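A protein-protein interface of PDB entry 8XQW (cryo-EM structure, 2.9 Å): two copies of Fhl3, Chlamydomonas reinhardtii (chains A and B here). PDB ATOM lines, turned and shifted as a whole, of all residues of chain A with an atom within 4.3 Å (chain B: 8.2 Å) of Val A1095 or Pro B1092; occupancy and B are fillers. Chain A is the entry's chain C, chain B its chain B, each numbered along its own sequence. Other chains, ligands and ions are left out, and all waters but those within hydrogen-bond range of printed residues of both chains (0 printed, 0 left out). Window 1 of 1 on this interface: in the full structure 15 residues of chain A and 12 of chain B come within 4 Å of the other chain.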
ATOM      1  N   TYR A1073      16.815  28.255  -3.102  1.00  0.00           N
ATOM      2  CA  TYR A1073      15.551  27.712  -2.626  1.00  0.00           C
ATOM      3  C   TYR A1073      14.900  26.770  -3.621  1.00  0.00           C
ATOM      4  O   TYR A1073      13.800  26.276  -3.364  1.00  0.00           O
ATOM      5  CB  TYR A1073      14.593  28.849  -2.291  1.00  0.00           C
ATOM      6  CG  TYR A1073      15.157  29.867  -1.351  1.00  0.00           C
ATOM      7  CD1 TYR A1073      15.098  29.677   0.010  1.00  0.00           C
ATOM      8  CD2 TYR A1073      15.746  31.021  -1.826  1.00  0.00           C
ATOM      9  CE1 TYR A1073      15.606  30.605   0.875  1.00  0.00           C
ATOM     10  CE2 TYR A1073      16.256  31.955  -0.970  1.00  0.00           C
ATOM     11  CZ  TYR A1073      16.186  31.743   0.380  1.00  0.00           C
ATOM     12  OH  TYR A1073      16.699  32.676   1.250  1.00  0.00           O
ATOM     13  N   ALA A1075      14.067  23.422  -5.818  1.00  0.00           N
ATOM     14  CA  ALA A1075      13.974  22.013  -5.484  1.00  0.00           C
ATOM     15  C   ALA A1075      15.026  21.214  -6.246  1.00  0.00           C
ATOM     16  O   ALA A1075      15.379  21.561  -7.371  1.00  0.00           O
ATOM     17  CB  ALA A1075      12.588  21.488  -5.816  1.00  0.00           C
ATOM     18  N   PRO A1076      15.543  20.142  -5.651  1.00  0.00           N
ATOM     19  CA  PRO A1076      16.604  19.379  -6.312  1.00  0.00           C
ATOM     20  C   PRO A1076      16.116  18.766  -7.612  1.00  0.00           C
ATOM     21  O   PRO A1076      15.005  18.247  -7.690  1.00  0.00           O
ATOM     22  CB  PRO A1076      16.955  18.306  -5.283  1.00  0.00           C
ATOM     23  CG  PRO A1076      15.758  18.194  -4.446  1.00  0.00           C
ATOM     24  CD  PRO A1076      15.176  19.553  -4.360  1.00  0.00           C
ATOM     25  N   TRP A1089       5.305  21.482  -7.992  1.00  0.00           N
ATOM     26  CA  TRP A1089       4.924  22.377  -6.906  1.00  0.00           C
ATOM     27  C   TRP A1089       3.460  22.242  -6.538  1.00  0.00           C
ATOM     28  O   TRP A1089       2.971  22.984  -5.686  1.00  0.00           O
ATOM     29  CB  TRP A1089       5.238  23.817  -7.274  1.00  0.00           C
ATOM     30  CG  TRP A1089       6.689  24.078  -7.410  1.00  0.00           C
ATOM     31  CD1 TRP A1089       7.466  23.780  -8.473  1.00  0.00           C
ATOM     32  CD2 TRP A1089       7.542  24.695  -6.451  1.00  0.00           C
ATOM     33  NE1 TRP A1089       8.752  24.164  -8.241  1.00  0.00           N
ATOM     34  CE2 TRP A1089       8.822  24.732  -7.000  1.00  0.00           C
ATOM     35  CE3 TRP A1089       7.345  25.215  -5.176  1.00  0.00           C
ATOM     36  CZ2 TRP A1089       9.897  25.265  -6.324  1.00  0.00           C
ATOM     37  CZ3 TRP A1089       8.410  25.747  -4.517  1.00  0.00           C
ATOM     38  CH2 TRP A1089       9.667  25.769  -5.086  1.00  0.00           C
ATOM     39  N   PHE A1093       3.023  17.668  -0.408  1.00  0.00           N
ATOM     40  CA  PHE A1093       4.080  17.413   0.553  1.00  0.00           C
ATOM     41  C   PHE A1093       5.376  17.998   0.026  1.00  0.00           C
ATOM     42  O   PHE A1093       5.616  17.993  -1.179  1.00  0.00           O
ATOM     43  CB  PHE A1093       4.253  15.925   0.784  1.00  0.00           C
ATOM     44  CG  PHE A1093       4.258  15.143  -0.476  1.00  0.00           C
ATOM     45  CD1 PHE A1093       5.410  15.014  -1.216  1.00  0.00           C
ATOM     46  CD2 PHE A1093       3.103  14.565  -0.948  1.00  0.00           C
ATOM     47  CE1 PHE A1093       5.417  14.307  -2.386  1.00  0.00           C
ATOM     48  CE2 PHE A1093       3.103  13.857  -2.123  1.00  0.00           C
ATOM     49  CZ  PHE A1093       4.263  13.728  -2.842  1.00  0.00           C
ATOM     50  N   SER A1094       6.212  18.490   0.930  1.00  0.00           N
ATOM     51  CA  SER A1094       7.443  19.126   0.510  1.00  0.00           C
ATOM     52  C   SER A1094       8.530  18.093   0.284  1.00  0.00           C
ATOM     53  O   SER A1094       8.420  16.936   0.680  1.00  0.00           O
ATOM     54  CB  SER A1094       7.907  20.137   1.543  1.00  0.00           C
ATOM     55  OG  SER A1094       6.837  20.957   1.949  1.00  0.00           O
ATOM     56  N   VAL A1095       9.592  18.537  -0.362  1.00  0.00           N
ATOM     57  CA  VAL A1095      10.746  17.700  -0.641  1.00  0.00           C
ATOM     58  C   VAL A1095      11.943  18.299   0.081  1.00  0.00           C
ATOM     59  O   VAL A1095      11.940  19.473   0.449  1.00  0.00           O
ATOM     60  CB  VAL A1095      10.978  17.593  -2.158  1.00  0.00           C
ATOM     61  CG1 VAL A1095      11.866  18.691  -2.632  1.00  0.00           C
ATOM     62  CG2 VAL A1095      11.544  16.254  -2.508  1.00  0.00           C
ATOM     63  N   LYS A1096      12.963  17.486   0.304  1.00  0.00           N
ATOM     64  CA  LYS A1096      14.100  17.907   1.107  1.00  0.00           C
ATOM     65  C   LYS A1096      15.284  18.265   0.224  1.00  0.00           C
ATOM     66  O   LYS A1096      15.711  17.459  -0.603  1.00  0.00           O
ATOM     67  CB  LYS A1096      14.500  16.806   2.080  1.00  0.00           C
ATOM     68  CG  LYS A1096      15.708  17.157   2.887  1.00  0.00           C
ATOM     69  CD  LYS A1096      16.114  16.020   3.773  1.00  0.00           C
ATOM     70  CE  LYS A1096      15.237  15.949   4.983  1.00  0.00           C
ATOM     71  NZ  LYS A1096      15.819  15.028   5.986  1.00  0.00           N
ATOM     72  N   THR A1097      15.814  19.466   0.408  1.00  0.00           N
ATOM     73  CA  THR A1097      16.991  19.885  -0.331  1.00  0.00           C
ATOM     74  C   THR A1097      18.205  19.097   0.133  1.00  0.00           C
ATOM     75  O   THR A1097      18.317  18.721   1.300  1.00  0.00           O
ATOM     76  CB  THR A1097      17.254  21.377  -0.140  1.00  0.00           C
ATOM     77  OG1 THR A1097      16.027  22.098  -0.251  1.00  0.00           O
ATOM     78  CG2 THR A1097      18.195  21.879  -1.199  1.00  0.00           C
ATOM     79  N   ARG B 906       3.156  19.314   6.309  1.00  0.00           N
ATOM     80  CA  ARG B 906       3.642  19.274   4.940  1.00  0.00           C
ATOM     81  C   ARG B 906       5.074  18.785   4.834  1.00  0.00           C
ATOM     82  O   ARG B 906       5.501  18.434   3.736  1.00  0.00           O
ATOM     83  CB  ARG B 906       3.526  20.650   4.296  1.00  0.00           C
ATOM     84  CG  ARG B 906       4.562  21.636   4.759  1.00  0.00           C
ATOM     85  CD  ARG B 906       4.485  22.910   3.970  1.00  0.00           C
ATOM     86  NE  ARG B 906       5.539  23.842   4.329  1.00  0.00           N
ATOM     87  CZ  ARG B 906       6.746  23.842   3.784  1.00  0.00           C
ATOM     88  NH1 ARG B 906       7.053  22.959   2.857  1.00  0.00           N
ATOM     89  NH2 ARG B 906       7.649  24.726   4.166  1.00  0.00           N
ATOM     90  N   ARG B 907       5.820  18.746   5.930  1.00  0.00           N
ATOM     91  CA  ARG B 907       7.224  18.373   5.873  1.00  0.00           C
ATOM     92  C   ARG B 907       7.504  16.952   6.320  1.00  0.00           C
ATOM     93  O   ARG B 907       8.435  16.340   5.806  1.00  0.00           O
ATOM     94  CB  ARG B 907       8.062  19.329   6.720  1.00  0.00           C
ATOM     95  CG  ARG B 907       8.386  20.605   6.014  1.00  0.00           C
ATOM     96  CD  ARG B 907       9.200  21.523   6.870  1.00  0.00           C
ATOM     97  NE  ARG B 907       8.368  22.282   7.782  1.00  0.00           N
ATOM     98  CZ  ARG B 907       8.616  23.532   8.134  1.00  0.00           C
ATOM     99  NH1 ARG B 907       9.668  24.159   7.639  1.00  0.00           N
ATOM    100  NH2 ARG B 907       7.808  24.156   8.974  1.00  0.00           N
ATOM    101  N   HIS B1088       6.349  30.629  -1.250  1.00  0.00           N
ATOM    102  CA  HIS B1088       5.417  29.607  -1.683  1.00  0.00           C
ATOM    103  C   HIS B1088       5.160  28.696  -0.496  1.00  0.00           C
ATOM    104  O   HIS B1088       6.037  28.487   0.335  1.00  0.00           O
ATOM    105  CB  HIS B1088       5.961  28.822  -2.873  1.00  0.00           C
ATOM    106  CG  HIS B1088       4.973  27.888  -3.485  1.00  0.00           C
ATOM    107  ND1 HIS B1088       4.046  28.289  -4.415  1.00  0.00           N
ATOM    108  CD2 HIS B1088       4.781  26.564  -3.316  1.00  0.00           C
ATOM    109  CE1 HIS B1088       3.313  27.255  -4.779  1.00  0.00           C
ATOM    110  NE2 HIS B1088       3.740  26.194  -4.129  1.00  0.00           N
ATOM    111  N   TRP B1089       3.949  28.170  -0.400  1.00  0.00           N
ATOM    112  CA  TRP B1089       3.634  27.370   0.770  1.00  0.00           C
ATOM    113  C   TRP B1089       4.335  26.027   0.773  1.00  0.00           C
ATOM    114  O   TRP B1089       4.164  25.275   1.730  1.00  0.00           O
ATOM    115  CB  TRP B1089       2.130  27.148   0.872  1.00  0.00           C
ATOM    116  CG  TRP B1089       1.576  26.279  -0.190  1.00  0.00           C
ATOM    117  CD1 TRP B1089       1.140  26.669  -1.405  1.00  0.00           C
ATOM    118  CD2 TRP B1089       1.385  24.869  -0.129  1.00  0.00           C
ATOM    119  NE1 TRP B1089       0.699  25.592  -2.118  1.00  0.00           N
ATOM    120  CE2 TRP B1089       0.842  24.471  -1.353  1.00  0.00           C
ATOM    121  CE3 TRP B1089       1.629  23.902   0.842  1.00  0.00           C
ATOM    122  CZ2 TRP B1089       0.537  23.159  -1.632  1.00  0.00           C
ATOM    123  CZ3 TRP B1089       1.328  22.601   0.559  1.00  0.00           C
ATOM    124  CH2 TRP B1089       0.787  22.240  -0.665  1.00  0.00           C
ATOM    125  N   ASN B1090       5.124  25.712  -0.241  1.00  0.00           N
ATOM    126  CA  ASN B1090       5.642  24.374  -0.469  1.00  0.00           C
ATOM    127  C   ASN B1090       7.120  24.422  -0.777  1.00  0.00           C
ATOM    128  O   ASN B1090       7.607  23.778  -1.701  1.00  0.00           O
ATOM    129  CB  ASN B1090       4.889  23.723  -1.615  1.00  0.00           C
ATOM    130  CG  ASN B1090       4.865  22.238  -1.524  1.00  0.00           C
ATOM    131  OD1 ASN B1090       5.138  21.675  -0.477  1.00  0.00           O
ATOM    132  ND2 ASN B1090       4.530  21.587  -2.617  1.00  0.00           N
ATOM    133  N   MET B1091       7.848  25.178  -0.019  1.00  0.00           N
ATOM    134  CA  MET B1091       9.266  25.311  -0.299  1.00  0.00           C
ATOM    135  C   MET B1091      10.033  24.123   0.263  1.00  0.00           C
ATOM    136  O   MET B1091       9.677  23.604   1.318  1.00  0.00           O
ATOM    137  CB  MET B1091       9.811  26.578   0.312  1.00  0.00           C
ATOM    138  CG  MET B1091       8.951  27.759   0.101  1.00  0.00           C
ATOM    139  SD  MET B1091       9.972  29.203  -0.039  1.00  0.00           S
ATOM    140  CE  MET B1091      11.267  28.536  -1.054  1.00  0.00           C
ATOM    141  N   PRO B1092      11.087  23.686  -0.410  1.00  0.00           N
ATOM    142  CA  PRO B1092      11.928  22.634   0.152  1.00  0.00           C
ATOM    143  C   PRO B1092      12.632  23.118   1.405  1.00  0.00           C
ATOM    144  O   PRO B1092      12.829  24.314   1.607  1.00  0.00           O
ATOM    145  CB  PRO B1092      12.924  22.347  -0.969  1.00  0.00           C
ATOM    146  CG  PRO B1092      12.300  22.893  -2.172  1.00  0.00           C
ATOM    147  CD  PRO B1092      11.541  24.076  -1.745  1.00  0.00           C
ATOM    148  N   PHE B1093      13.016  22.173   2.255  1.00  0.00           N
ATOM    149  CA  PHE B1093      13.654  22.483   3.521  1.00  0.00           C
ATOM    150  C   PHE B1093      14.950  21.701   3.635  1.00  0.00           C
ATOM    151  O   PHE B1093      15.355  20.995   2.714  1.00  0.00           O
ATOM    152  CB  PHE B1093      12.736  22.167   4.700  1.00  0.00           C
ATOM    153  CG  PHE B1093      12.378  20.730   4.808  1.00  0.00           C
ATOM    154  CD1 PHE B1093      11.367  20.204   4.049  1.00  0.00           C
ATOM    155  CD2 PHE B1093      13.049  19.903   5.671  1.00  0.00           C
ATOM    156  CE1 PHE B1093      11.039  18.889   4.148  1.00  0.00           C
ATOM    157  CE2 PHE B1093      12.720  18.584   5.770  1.00  0.00           C
ATOM    158  CZ  PHE B1093      11.717  18.078   5.009  1.00  0.00           C
ATOM    159  N   SER B1094      15.608  21.836   4.780  1.00  0.00           N
ATOM    160  CA  SER B1094      16.867  21.149   5.014  1.00  0.00           C
ATOM    161  C   SER B1094      17.173  21.167   6.500  1.00  0.00           C
ATOM    162  O   SER B1094      16.678  22.012   7.242  1.00  0.00           O
ATOM    163  CB  SER B1094      18.001  21.795   4.230  1.00  0.00           C
ATOM    164  OG  SER B1094      17.797  23.190   4.144  1.00  0.00           O
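Of the 9 printed residues of chain B, 6 touch a printed residue of chain A. Printed residues of chain B that touch a printed residue of chain A: Arg B906, His B1088, Asn B1090, Met B1091, Pro B1092 and Phe B1093. Hydrophobic or aromatic side chains of chain B that line the printed part of chain A: His B1088, Met B1091, Pro B1092 and Phe B1093. Along chain A the printed residues that touch a printed residue of chain B span positions 1073 to 1097.
Positions printed for both chains: 1089, 1093 and 1094.
Of the printed residues of chain B, Ala A1075 touches Pro B1092 (3.8 Å). Printed residues of chain B within 4 Å of Ser A1094: Arg B906 (2.2 Å), Asn B1090 (3.0 Å) and Met B1091 (3.9 Å). Of the printed residues of chain B, Val A1095 touches Pro B1092 (3.2 Å) and Phe B1093 (3.4 Å). Trp B1089 touches none of the printed residues of chain A. Printed residues of chain A within 4 Å of Pro B1092: Tyr A1073 (3.5 Å), Ala A1075 (3.8 Å), Val A1095 (3.2 Å) and Thr A1097 (3.2 Å). The nearest residue of chain A that does not touch Pro B1092 is Trp A1089 (4.2 Å). The nearest printed residue of chain B that does not touch Thr A1097 is Ser B1094 (4.3 Å).
CD of Pro B1092 touches O of Tyr A1073 (3.5 Å). CA of Ala A1075 touches CG of Pro B1092, 3.8 Å away. His B1088 touches Trp A1089 (CD2 to CE3, 3.4 Å). Trp A1089 touches Asn B1090. Arg B906 touches Phe A1093. Asn B1090 touches Phe A1093 (OD1 to C, 3.7 Å). CB of Ser A1094 touches O of Met B1091 (3.9 Å). Pro B1092 touches Val A1095. C of Lys A1096 touches O of Phe B1093 (3.7 Å). Thr A1097 touches Pro B1092.
The backbone carbonyl oxygen of Trp B1089 is in hydrogen-bond range of the guanidinium group of Arg B906, at 3.3 Å. O of Met B1091 lies within hydrogen-bond range of NH1 of Arg B906, at 3.1 Å.
The backbone carbonyl oxygen (O) of Arg B906 sits at hydrogen-bond distance from the backbone NH (N) of Ser A1094 (2.9 Å). OD1 of Asn B1090 lies within hydrogen-bond range of OG of Ser A1094 (3.0 Å). N of Phe B1093 lies within hydrogen-bond range of O of Val A1095, at 3.4 Å. The backbone carbonyl oxygen of Phe B1093 sits at hydrogen-bond distance from the backbone NH of Thr A1097, 2.8 Å away.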
